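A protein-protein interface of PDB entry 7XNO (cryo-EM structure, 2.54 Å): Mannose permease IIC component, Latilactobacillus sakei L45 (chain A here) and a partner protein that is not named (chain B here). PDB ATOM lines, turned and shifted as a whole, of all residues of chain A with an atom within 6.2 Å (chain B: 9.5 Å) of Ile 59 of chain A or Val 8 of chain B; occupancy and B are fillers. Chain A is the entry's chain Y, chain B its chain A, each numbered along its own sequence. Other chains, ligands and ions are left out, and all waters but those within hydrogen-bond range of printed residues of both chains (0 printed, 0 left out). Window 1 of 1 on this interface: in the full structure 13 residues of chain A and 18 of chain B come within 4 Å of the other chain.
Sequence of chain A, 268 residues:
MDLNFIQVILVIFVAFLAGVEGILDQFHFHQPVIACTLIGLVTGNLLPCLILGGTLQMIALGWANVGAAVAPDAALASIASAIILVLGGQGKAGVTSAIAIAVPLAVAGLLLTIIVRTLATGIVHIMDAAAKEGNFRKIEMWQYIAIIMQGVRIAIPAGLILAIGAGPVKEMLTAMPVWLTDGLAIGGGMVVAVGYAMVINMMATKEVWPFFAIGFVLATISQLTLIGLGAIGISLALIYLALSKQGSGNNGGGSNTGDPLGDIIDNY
Among the printed residues, merely in contact across the chains: Met 58 of chain A with Ala 22 of chain B (3.7 Å), Met 58 of chain A with Val 17 of chain B (3.7 Å), Thr 55 of chain A with Val 8 of chain B (3.8 Å), Met 58 of chain A with Val 8 of chain B (3.8 Å), Leu 61 of chain A with Asn 6 of chain B (3.9 Å), Ile 59 of chain A with Val 8 of chain B (3.9 Å), Met 58 of chain A with Arg 19 of chain B (3.9 Å) and Ile 99 of chain A with Cys 10 of chain B (3.9 Å).
Of chain B, only Asn 6 and Val 8 come within 4 Å of Ile 59 of chain A. No residue of chain B comes within 4 Å of Ala 60 of chain A. Ala 1 of chain B touches none of the printed residues of chain A. Arg 2 of chain B touches none of the printed residues of chain A. Val 8 of chain B touches three residues of chain A. Printed residues of chain A within 4 Å of Val 17 of chain B: Met 58 (3.7 Å). Of the printed residues of chain A, Ala 22 of chain B touches Met 58 (3.7 Å). The nearest residue of chain B that does not touch Ile 59 of chain A is Tyr 4 of chain B (4.02 Å). The nearest residue of chain A that does not touch Val 8 of chain B is Ile 99 of chain A (5.6 Å).
Of the 22 printed residues of chain B, 6 touch a printed residue of chain A. Hydrophobic or aromatic side chains of chain B that line the printed part of chain A: Val 8, Val 17 and Ala 22. Along chain A the printed residues that touch a printed residue of chain B span positions 55 to 99. Among the printed residues, 10 pairs touch across the chains. Among the printed residues, no Asp or Glu carboxylate lies within 4 Å of a Lys or Arg side-chain nitrogen of the other chain.
The backbone carbonyl oxygen (O) of Met 58 of chain A lies within hydrogen-bond range of the side-chain amide nitrogen (ND2) of Asn 6 of chain B (2.7 Å). The side-chain amide nitrogen (ND2) of Asn 6 of chain B sits at hydrogen-bond distance from the backbone carbonyl oxygen (O) of Ile 59 of chain A, 3.0 Å away.
O of Arg 2 of chain B lies within hydrogen-bond range of N of Cys 10 of chain B (3.2 Å). The side-chain sulfur (SG) of Cys 10 of chain B is disulfide-bonded to the side-chain sulfur (SG) of Cys 15 of chain B (2.0 Å). The backbone carbonyl oxygen (O) of Arg 19 of chain B sits at hydrogen-bond distance from the side-chain hydroxyl (OG1) of Thr 23 of chain B, 2.9 Å away.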
ATOM      1  N   GLY A  54      -0.283  22.502 -14.806  1.00  0.00           N
ATOM      2  CA  GLY A  54      -1.654  22.449 -14.325  1.00  0.00           C
ATOM      3  C   GLY A  54      -1.969  23.572 -13.356  1.00  0.00           C
ATOM      4  O   GLY A  54      -3.007  24.235 -13.464  1.00  0.00           O
ATOM      5  N   THR A  55      -1.065  23.816 -12.404  1.00  0.00           N
ATOM      6  CA  THR A  55      -1.297  24.878 -11.428  1.00  0.00           C
ATOM      7  C   THR A  55      -1.362  26.247 -12.099  1.00  0.00           C
ATOM      8  O   THR A  55      -2.249  27.056 -11.797  1.00  0.00           O
ATOM      9  CB  THR A  55      -0.203  24.861 -10.359  1.00  0.00           C
ATOM     10  OG1 THR A  55       0.008  23.517  -9.911  1.00  0.00           O
ATOM     11  CG2 THR A  55      -0.602  25.725  -9.176  1.00  0.00           C
ATOM     12  N   LEU A  56      -0.440  26.519 -13.024  1.00  0.00           N
ATOM     13  CA  LEU A  56      -0.419  27.818 -13.684  1.00  0.00           C
ATOM     14  C   LEU A  56      -1.607  27.991 -14.623  1.00  0.00           C
ATOM     15  O   LEU A  56      -2.133  29.101 -14.749  1.00  0.00           O
ATOM     16  CB  LEU A  56       0.899  28.002 -14.435  1.00  0.00           C
ATOM     17  CG  LEU A  56       1.169  29.389 -15.016  1.00  0.00           C
ATOM     18  CD1 LEU A  56       1.005  30.454 -13.949  1.00  0.00           C
ATOM     19  CD2 LEU A  56       2.563  29.445 -15.606  1.00  0.00           C
ATOM     20  N   GLN A  57      -2.045  26.915 -15.283  1.00  0.00           N
ATOM     21  CA  GLN A  57      -3.251  26.984 -16.096  1.00  0.00           C
ATOM     22  C   GLN A  57      -4.467  27.292 -15.237  1.00  0.00           C
ATOM     23  O   GLN A  57      -5.352  28.050 -15.650  1.00  0.00           O
ATOM     24  CB  GLN A  57      -3.450  25.672 -16.852  1.00  0.00           C
ATOM     25  CG  GLN A  57      -4.735  25.601 -17.657  1.00  0.00           C
ATOM     26  CD  GLN A  57      -4.677  26.427 -18.923  1.00  0.00           C
ATOM     27  OE1 GLN A  57      -3.744  26.302 -19.714  1.00  0.00           O
ATOM     28  NE2 GLN A  57      -5.675  27.278 -19.121  1.00  0.00           N
ATOM     29  N   MET A  58      -4.532  26.707 -14.040  1.00  0.00           N
ATOM     30  CA  MET A  58      -5.594  27.075 -13.113  1.00  0.00           C
ATOM     31  C   MET A  58      -5.498  28.549 -12.737  1.00  0.00           C
ATOM     32  O   MET A  58      -6.519  29.237 -12.619  1.00  0.00           O
ATOM     33  CB  MET A  58      -5.534  26.195 -11.866  1.00  0.00           C
ATOM     34  CG  MET A  58      -6.890  25.907 -11.257  1.00  0.00           C
ATOM     35  SD  MET A  58      -7.886  24.823 -12.294  1.00  0.00           S
ATOM     36  CE  MET A  58      -9.520  25.490 -12.004  1.00  0.00           C
ATOM     37  N   ILE A  59      -4.276  29.052 -12.548  1.00  0.00           N
ATOM     38  CA  ILE A  59      -4.093  30.470 -12.254  1.00  0.00           C
ATOM     39  C   ILE A  59      -4.471  31.328 -13.459  1.00  0.00           C
ATOM     40  O   ILE A  59      -5.098  32.384 -13.314  1.00  0.00           O
ATOM     41  CB  ILE A  59      -2.645  30.733 -11.800  1.00  0.00           C
ATOM     42  CG1 ILE A  59      -2.436  30.238 -10.370  1.00  0.00           C
ATOM     43  CG2 ILE A  59      -2.299  32.211 -11.908  1.00  0.00           C
ATOM     44  CD1 ILE A  59      -0.983  30.098  -9.986  1.00  0.00           C
ATOM     45  N   ALA A  60      -4.113  30.883 -14.664  1.00  0.00           N
ATOM     46  CA  ALA A  60      -4.215  31.694 -15.872  1.00  0.00           C
ATOM     47  C   ALA A  60      -5.456  31.377 -16.702  1.00  0.00           C
ATOM     48  O   ALA A  60      -5.435  31.533 -17.926  1.00  0.00           O
ATOM     49  CB  ALA A  60      -2.957  31.521 -16.723  1.00  0.00           C
ATOM     50  N   LEU A  61      -6.541  30.931 -16.063  1.00  0.00           N
ATOM     51  CA  LEU A  61      -7.751  30.604 -16.812  1.00  0.00           C
ATOM     52  C   LEU A  61      -8.361  31.837 -17.468  1.00  0.00           C
ATOM     53  O   LEU A  61      -8.819  31.772 -18.615  1.00  0.00           O
ATOM     54  CB  LEU A  61      -8.777  29.935 -15.897  1.00  0.00           C
ATOM     55  CG  LEU A  61      -8.582  28.454 -15.580  1.00  0.00           C
ATOM     56  CD1 LEU A  61      -9.694  27.969 -14.670  1.00  0.00           C
ATOM     57  CD2 LEU A  61      -8.535  27.635 -16.855  1.00  0.00           C
ATOM     58  N   GLY A  62      -8.381  32.963 -16.763  1.00  0.00           N
ATOM     59  CA  GLY A  62      -9.092  34.135 -17.235  1.00  0.00           C
ATOM     60  C   GLY A  62      -8.253  35.144 -17.990  1.00  0.00           C
ATOM     61  O   GLY A  62      -8.669  36.293 -18.157  1.00  0.00           O
ATOM     62  N   TRP A  63      -7.073  34.737 -18.453  1.00  0.00           N
ATOM     63  CA  TRP A  63      -6.182  35.637 -19.184  1.00  0.00           C
ATOM     64  C   TRP A  63      -6.600  35.627 -20.648  1.00  0.00           C
ATOM     65  O   TRP A  63      -6.165  34.787 -21.438  1.00  0.00           O
ATOM     66  CB  TRP A  63      -4.727  35.227 -19.006  1.00  0.00           C
ATOM     67  CG  TRP A  63      -4.223  35.418 -17.608  1.00  0.00           C
ATOM     68  CD1 TRP A  63      -4.917  35.921 -16.548  1.00  0.00           C
ATOM     69  CD2 TRP A  63      -2.912  35.114 -17.120  1.00  0.00           C
ATOM     70  NE1 TRP A  63      -4.124  35.944 -15.430  1.00  0.00           N
ATOM     71  CE2 TRP A  63      -2.887  35.455 -15.754  1.00  0.00           C
ATOM     72  CE3 TRP A  63      -1.757  34.588 -17.705  1.00  0.00           C
ATOM     73  CZ2 TRP A  63      -1.754  35.283 -14.965  1.00  0.00           C
ATOM     74  CZ3 TRP A  63      -0.635  34.418 -16.919  1.00  0.00           C
ATOM     75  CH2 TRP A  63      -0.641  34.763 -15.565  1.00  0.00           C
ATOM     76  N   ILE A  99       5.619  29.076  -9.151  1.00  0.00           N
ATOM     77  CA  ILE A  99       4.311  29.721  -9.150  1.00  0.00           C
ATOM     78  C   ILE A  99       4.419  31.136  -8.597  1.00  0.00           C
ATOM     79  O   ILE A  99       3.768  32.065  -9.091  1.00  0.00           O
ATOM     80  CB  ILE A  99       3.302  28.871  -8.357  1.00  0.00           C
ATOM     81  CG1 ILE A  99       2.879  27.652  -9.177  1.00  0.00           C
ATOM     82  CG2 ILE A  99       2.087  29.695  -7.960  1.00  0.00           C
ATOM     83  CD1 ILE A  99       2.102  27.997 -10.426  1.00  0.00           C
ATOM     84  N   VAL A 103       3.785  35.096 -11.966  1.00  0.00           N
ATOM     85  CA  VAL A 103       2.912  36.246 -12.209  1.00  0.00           C
ATOM     86  C   VAL A 103       3.705  37.507 -12.554  1.00  0.00           C
ATOM     87  O   VAL A 103       3.332  38.213 -13.506  1.00  0.00           O
ATOM     88  CB  VAL A 103       1.970  36.483 -11.015  1.00  0.00           C
ATOM     89  CG1 VAL A 103       0.857  37.441 -11.403  1.00  0.00           C
ATOM     90  CG2 VAL A 103       1.392  35.161 -10.530  1.00  0.00           C
ATOM     91  N   ALA B   1      -1.122  30.370   4.029  1.00  0.00           N
ATOM     92  CA  ALA B   1      -1.359  30.020   2.634  1.00  0.00           C
ATOM     93  C   ALA B   1      -1.550  31.269   1.784  1.00  0.00           C
ATOM     94  O   ALA B   1      -2.307  32.168   2.146  1.00  0.00           O
ATOM     95  CB  ALA B   1      -2.569  29.108   2.515  1.00  0.00           C
ATOM     96  N   ARG B   2      -0.857  31.319   0.651  1.00  0.00           N
ATOM     97  CA  ARG B   2      -0.933  32.453  -0.257  1.00  0.00           C
ATOM     98  C   ARG B   2      -1.970  32.179  -1.338  1.00  0.00           C
ATOM     99  O   ARG B   2      -1.925  31.138  -2.000  1.00  0.00           O
ATOM    100  CB  ARG B   2       0.430  32.728  -0.891  1.00  0.00           C
ATOM    101  CG  ARG B   2       1.446  33.328   0.059  1.00  0.00           C
ATOM    102  CD  ARG B   2       2.791  33.501  -0.618  1.00  0.00           C
ATOM    103  NE  ARG B   2       3.222  32.288  -1.300  1.00  0.00           N
ATOM    104  CZ  ARG B   2       4.114  31.433  -0.817  1.00  0.00           C
ATOM    105  NH1 ARG B   2       4.689  31.625   0.358  1.00  0.00           N
ATOM    106  NH2 ARG B   2       4.437  30.360  -1.532  1.00  0.00           N
ATOM    107  N   SER B   3      -2.897  33.115  -1.516  1.00  0.00           N
ATOM    108  CA  SER B   3      -3.925  32.999  -2.539  1.00  0.00           C
ATOM    109  C   SER B   3      -3.409  33.546  -3.862  1.00  0.00           C
ATOM    110  O   SER B   3      -2.770  34.601  -3.906  1.00  0.00           O
ATOM    111  CB  SER B   3      -5.191  33.747  -2.120  1.00  0.00           C
ATOM    112  OG  SER B   3      -6.260  33.473  -3.007  1.00  0.00           O
ATOM    113  N   TYR B   4      -3.690  32.818  -4.945  1.00  0.00           N
ATOM    114  CA  TYR B   4      -3.220  33.199  -6.270  1.00  0.00           C
ATOM    115  C   TYR B   4      -4.346  33.314  -7.290  1.00  0.00           C
ATOM    116  O   TYR B   4      -4.068  33.417  -8.490  1.00  0.00           O
ATOM    117  CB  TYR B   4      -2.165  32.205  -6.769  1.00  0.00           C
ATOM    118  CG  TYR B   4      -0.817  32.379  -6.114  1.00  0.00           C
ATOM    119  CD1 TYR B   4       0.044  33.391  -6.511  1.00  0.00           C
ATOM    120  CD2 TYR B   4      -0.407  31.536  -5.090  1.00  0.00           C
ATOM    121  CE1 TYR B   4       1.275  33.557  -5.913  1.00  0.00           C
ATOM    122  CE2 TYR B   4       0.823  31.693  -4.486  1.00  0.00           C
ATOM    123  CZ  TYR B   4       1.660  32.706  -4.901  1.00  0.00           C
ATOM    124  OH  TYR B   4       2.887  32.867  -4.303  1.00  0.00           O
ATOM    125  N   GLY B   5      -5.595  33.300  -6.855  1.00  0.00           N
ATOM    126  CA  GLY B   5      -6.702  33.449  -7.785  1.00  0.00           C
ATOM    127  C   GLY B   5      -7.216  32.118  -8.295  1.00  0.00           C
ATOM    128  O   GLY B   5      -6.486  31.134  -8.406  1.00  0.00           O
ATOM    129  N   ASN B   6      -8.512  32.097  -8.612  1.00  0.00           N
ATOM    130  CA  ASN B   6      -9.199  30.905  -9.111  1.00  0.00           C
ATOM    131  C   ASN B   6      -9.118  29.746  -8.121  1.00  0.00           C
ATOM    132  O   ASN B   6      -9.146  28.577  -8.513  1.00  0.00           O
ATOM    133  CB  ASN B   6      -8.659  30.478 -10.479  1.00  0.00           C
ATOM    134  CG  ASN B   6      -8.819  31.556 -11.531  1.00  0.00           C
ATOM    135  OD1 ASN B   6      -9.750  32.359 -11.475  1.00  0.00           O
ATOM    136  ND2 ASN B   6      -7.910  31.581 -12.496  1.00  0.00           N
ATOM    137  N   GLY B   7      -9.020  30.062  -6.831  1.00  0.00           N
ATOM    138  CA  GLY B   7      -8.971  29.033  -5.813  1.00  0.00           C
ATOM    139  C   GLY B   7      -7.652  28.307  -5.692  1.00  0.00           C
ATOM    140  O   GLY B   7      -7.624  27.186  -5.182  1.00  0.00           O
ATOM    141  N   VAL B   8      -6.556  28.912  -6.136  1.00  0.00           N
ATOM    142  CA  VAL B   8      -5.238  28.290  -6.090  1.00  0.00           C
ATOM    143  C   VAL B   8      -4.481  28.852  -4.894  1.00  0.00           C
ATOM    144  O   VAL B   8      -4.334  30.073  -4.760  1.00  0.00           O
ATOM    145  CB  VAL B   8      -4.459  28.524  -7.394  1.00  0.00           C
ATOM    146  CG1 VAL B   8      -3.106  27.837  -7.332  1.00  0.00           C
ATOM    147  CG2 VAL B   8      -5.260  28.027  -8.585  1.00  0.00           C
ATOM    148  N   TYR B   9      -3.999  27.963  -4.027  1.00  0.00           N
ATOM    149  CA  TYR B   9      -3.245  28.343  -2.840  1.00  0.00           C
ATOM    150  C   TYR B   9      -1.933  27.576  -2.819  1.00  0.00           C
ATOM    151  O   TYR B   9      -1.827  26.500  -3.413  1.00  0.00           O
ATOM    152  CB  TYR B   9      -4.034  28.061  -1.561  1.00  0.00           C
ATOM    153  CG  TYR B   9      -5.305  28.863  -1.435  1.00  0.00           C
ATOM    154  CD1 TYR B   9      -6.471  28.451  -2.063  1.00  0.00           C
ATOM    155  CD2 TYR B   9      -5.342  30.029  -0.687  1.00  0.00           C
ATOM    156  CE1 TYR B   9      -7.635  29.178  -1.950  1.00  0.00           C
ATOM    157  CE2 TYR B   9      -6.502  30.764  -0.569  1.00  0.00           C
ATOM    158  CZ  TYR B   9      -7.646  30.334  -1.204  1.00  0.00           C
ATOM    159  OH  TYR B   9      -8.808  31.061  -1.091  1.00  0.00           O
ATOM    160  N   CYS B  10      -0.930  28.136  -2.148  1.00  0.00           N
ATOM    161  CA  CYS B  10       0.389  27.521  -2.076  1.00  0.00           C
ATOM    162  C   CYS B  10       1.015  27.767  -0.711  1.00  0.00           C
ATOM    163  O   CYS B  10       1.043  28.906  -0.234  1.00  0.00           O
ATOM    164  CB  CYS B  10       1.310  28.057  -3.178  1.00  0.00           C
ATOM    165  SG  CYS B  10       0.826  27.601  -4.861  1.00  0.00           S
ATOM    166  N   ASN B  11       1.512  26.699  -0.091  1.00  0.00           N
ATOM    167  CA  ASN B  11       2.382  26.812   1.073  1.00  0.00           C
ATOM    168  C   ASN B  11       3.810  27.059   0.598  1.00  0.00           C
ATOM    169  O   ASN B  11       4.062  27.368  -0.570  1.00  0.00           O
ATOM    170  CB  ASN B  11       2.307  25.561   1.945  1.00  0.00           C
ATOM    171  CG  ASN B  11       0.969  25.394   2.628  1.00  0.00           C
ATOM    172  OD1 ASN B  11       0.310  24.368   2.480  1.00  0.00           O
ATOM    173  ND2 ASN B  11       0.559  26.405   3.383  1.00  0.00           N
ATOM    174  N   LYS B  14       3.925  23.197  -0.993  1.00  0.00           N
ATOM    175  CA  LYS B  14       2.851  22.524  -1.710  1.00  0.00           C
ATOM    176  C   LYS B  14       1.885  23.554  -2.279  1.00  0.00           C
ATOM    177  O   LYS B  14       1.670  24.615  -1.689  1.00  0.00           O
ATOM    178  CB  LYS B  14       2.104  21.549  -0.788  1.00  0.00           C
ATOM    179  CG  LYS B  14       1.031  20.718  -1.470  1.00  0.00           C
ATOM    180  CD  LYS B  14       0.402  19.726  -0.507  1.00  0.00           C
ATOM    181  CE  LYS B  14      -0.674  18.902  -1.191  1.00  0.00           C
ATOM    182  NZ  LYS B  14      -1.308  17.924  -0.264  1.00  0.00           N
ATOM    183  N   CYS B  15       1.307  23.226  -3.433  1.00  0.00           N
ATOM    184  CA  CYS B  15       0.244  24.009  -4.049  1.00  0.00           C
ATOM    185  C   CYS B  15      -0.977  23.128  -4.264  1.00  0.00           C
ATOM    186  O   CYS B  15      -0.852  21.935  -4.556  1.00  0.00           O
ATOM    187  CB  CYS B  15       0.686  24.616  -5.388  1.00  0.00           C
ATOM    188  SG  CYS B  15       1.915  25.935  -5.267  1.00  0.00           S
ATOM    189  N   TRP B  16      -2.160  23.721  -4.116  1.00  0.00           N
ATOM    190  CA  TRP B  16      -3.411  23.002  -4.307  1.00  0.00           C
ATOM    191  C   TRP B  16      -4.470  23.973  -4.805  1.00  0.00           C
ATOM    192  O   TRP B  16      -4.254  25.187  -4.859  1.00  0.00           O
ATOM    193  CB  TRP B  16      -3.871  22.315  -3.016  1.00  0.00           C
ATOM    194  CG  TRP B  16      -4.277  23.268  -1.937  1.00  0.00           C
ATOM    195  CD1 TRP B  16      -5.542  23.676  -1.637  1.00  0.00           C
ATOM    196  CD2 TRP B  16      -3.410  23.946  -1.024  1.00  0.00           C
ATOM    197  NE1 TRP B  16      -5.518  24.560  -0.587  1.00  0.00           N
ATOM    198  CE2 TRP B  16      -4.218  24.743  -0.193  1.00  0.00           C
ATOM    199  CE3 TRP B  16      -2.026  23.955  -0.827  1.00  0.00           C
ATOM    200  CZ2 TRP B  16      -3.690  25.538   0.819  1.00  0.00           C
ATOM    201  CZ3 TRP B  16      -1.507  24.744   0.172  1.00  0.00           C
ATOM    202  CH2 TRP B  16      -2.334  25.526   0.985  1.00  0.00           C
ATOM    203  N   VAL B  17      -5.619  23.421  -5.183  1.00  0.00           N
ATOM    204  CA  VAL B  17      -6.728  24.191  -5.732  1.00  0.00           C
ATOM    205  C   VAL B  17      -7.982  23.887  -4.926  1.00  0.00           C
ATOM    206  O   VAL B  17      -8.315  22.718  -4.703  1.00  0.00           O
ATOM    207  CB  VAL B  17      -6.953  23.882  -7.224  1.00  0.00           C
ATOM    208  CG1 VAL B  17      -8.283  24.446  -7.694  1.00  0.00           C
ATOM    209  CG2 VAL B  17      -5.815  24.441  -8.056  1.00  0.00           C
ATOM    210  N   ASN B  18      -8.669  24.938  -4.486  1.00  0.00           N
ATOM    211  CA  ASN B  18      -9.990  24.797  -3.888  1.00  0.00           C
ATOM    212  C   ASN B  18     -11.017  24.662  -5.004  1.00  0.00           C
ATOM    213  O   ASN B  18     -11.193  25.586  -5.806  1.00  0.00           O
ATOM    214  CB  ASN B  18     -10.302  26.000  -2.999  1.00  0.00           C
ATOM    215  CG  ASN B  18     -11.499  25.770  -2.098  1.00  0.00           C
ATOM    216  OD1 ASN B  18     -12.400  24.997  -2.421  1.00  0.00           O
ATOM    217  ND2 ASN B  18     -11.516  26.450  -0.959  1.00  0.00           N
ATOM    218  N   ARG B  19     -11.689  23.509  -5.064  1.00  0.00           N
ATOM    219  CA  ARG B  19     -12.578  23.234  -6.189  1.00  0.00           C
ATOM    220  C   ARG B  19     -13.799  24.144  -6.179  1.00  0.00           C
ATOM    221  O   ARG B  19     -14.251  24.594  -7.238  1.00  0.00           O
ATOM    222  CB  ARG B  19     -13.001  21.766  -6.178  1.00  0.00           C
ATOM    223  CG  ARG B  19     -11.878  20.795  -6.510  1.00  0.00           C
ATOM    224  CD  ARG B  19     -11.232  21.119  -7.849  1.00  0.00           C
ATOM    225  NE  ARG B  19     -12.213  21.303  -8.913  1.00  0.00           N
ATOM    226  CZ  ARG B  19     -11.924  21.743 -10.130  1.00  0.00           C
ATOM    227  NH1 ARG B  19     -10.684  22.044 -10.480  1.00  0.00           N
ATOM    228  NH2 ARG B  19     -12.902  21.883 -11.019  1.00  0.00           N
ATOM    229  N   GLY B  20     -14.354  24.422  -4.998  1.00  0.00           N
ATOM    230  CA  GLY B  20     -15.512  25.301  -4.931  1.00  0.00           C
ATOM    231  C   GLY B  20     -15.191  26.715  -5.373  1.00  0.00           C
ATOM    232  O   GLY B  20     -15.937  27.328  -6.142  1.00  0.00           O
ATOM    233  N   GLU B  21     -14.065  27.251  -4.895  1.00  0.00           N
ATOM    234  CA  GLU B  21     -13.651  28.587  -5.307  1.00  0.00           C
ATOM    235  C   GLU B  21     -13.315  28.627  -6.791  1.00  0.00           C
ATOM    236  O   GLU B  21     -13.604  29.618  -7.468  1.00  0.00           O
ATOM    237  CB  GLU B  21     -12.463  29.054  -4.470  1.00  0.00           C
ATOM    238  CG  GLU B  21     -12.847  29.553  -3.089  1.00  0.00           C
ATOM    239  CD  GLU B  21     -11.690  30.200  -2.359  1.00  0.00           C
ATOM    240  OE1 GLU B  21     -11.938  30.945  -1.389  1.00  0.00           O
ATOM    241  OE2 GLU B  21     -10.531  29.966  -2.758  1.00  0.00           O
ATOM    242  N   ALA B  22     -12.703  27.563  -7.316  1.00  0.00           N
ATOM    243  CA  ALA B  22     -12.414  27.509  -8.746  1.00  0.00           C
ATOM    244  C   ALA B  22     -13.695  27.510  -9.571  1.00  0.00           C
ATOM    245  O   ALA B  22     -13.789  28.210 -10.588  1.00  0.00           O
ATOM    246  CB  ALA B  22     -11.572  26.275  -9.061  1.00  0.00           C
ATOM    247  N   THR B  23     -14.692  26.729  -9.150  1.00  0.00           N
ATOM    248  CA  THR B  23     -15.968  26.706  -9.858  1.00  0.00           C
ATOM    249  C   THR B  23     -16.650  28.066  -9.803  1.00  0.00           C
ATOM    250  O   THR B  23     -17.198  28.538 -10.808  1.00  0.00           O
ATOM    251  CB  THR B  23     -16.874  25.625  -9.266  1.00  0.00           C
ATOM    252  OG1 THR B  23     -16.240  24.346  -9.397  1.00  0.00           O
ATOM    253  CG2 THR B  23     -18.214  25.592  -9.984  1.00  0.00           C
ATOM    254  N   SER B  25     -15.162  30.956  -9.464  1.00  0.00           N
ATOM    255  CA  SER B  25     -14.397  31.847 -10.328  1.00  0.00           C
ATOM    256  C   SER B  25     -14.760  31.640 -11.790  1.00  0.00           C
ATOM    257  O   SER B  25     -14.935  32.610 -12.536  1.00  0.00           O
ATOM    258  CB  SER B  25     -12.901  31.632 -10.109  1.00  0.00           C
ATOM    259  OG  SER B  25     -12.506  32.076  -8.823  1.00  0.00           O
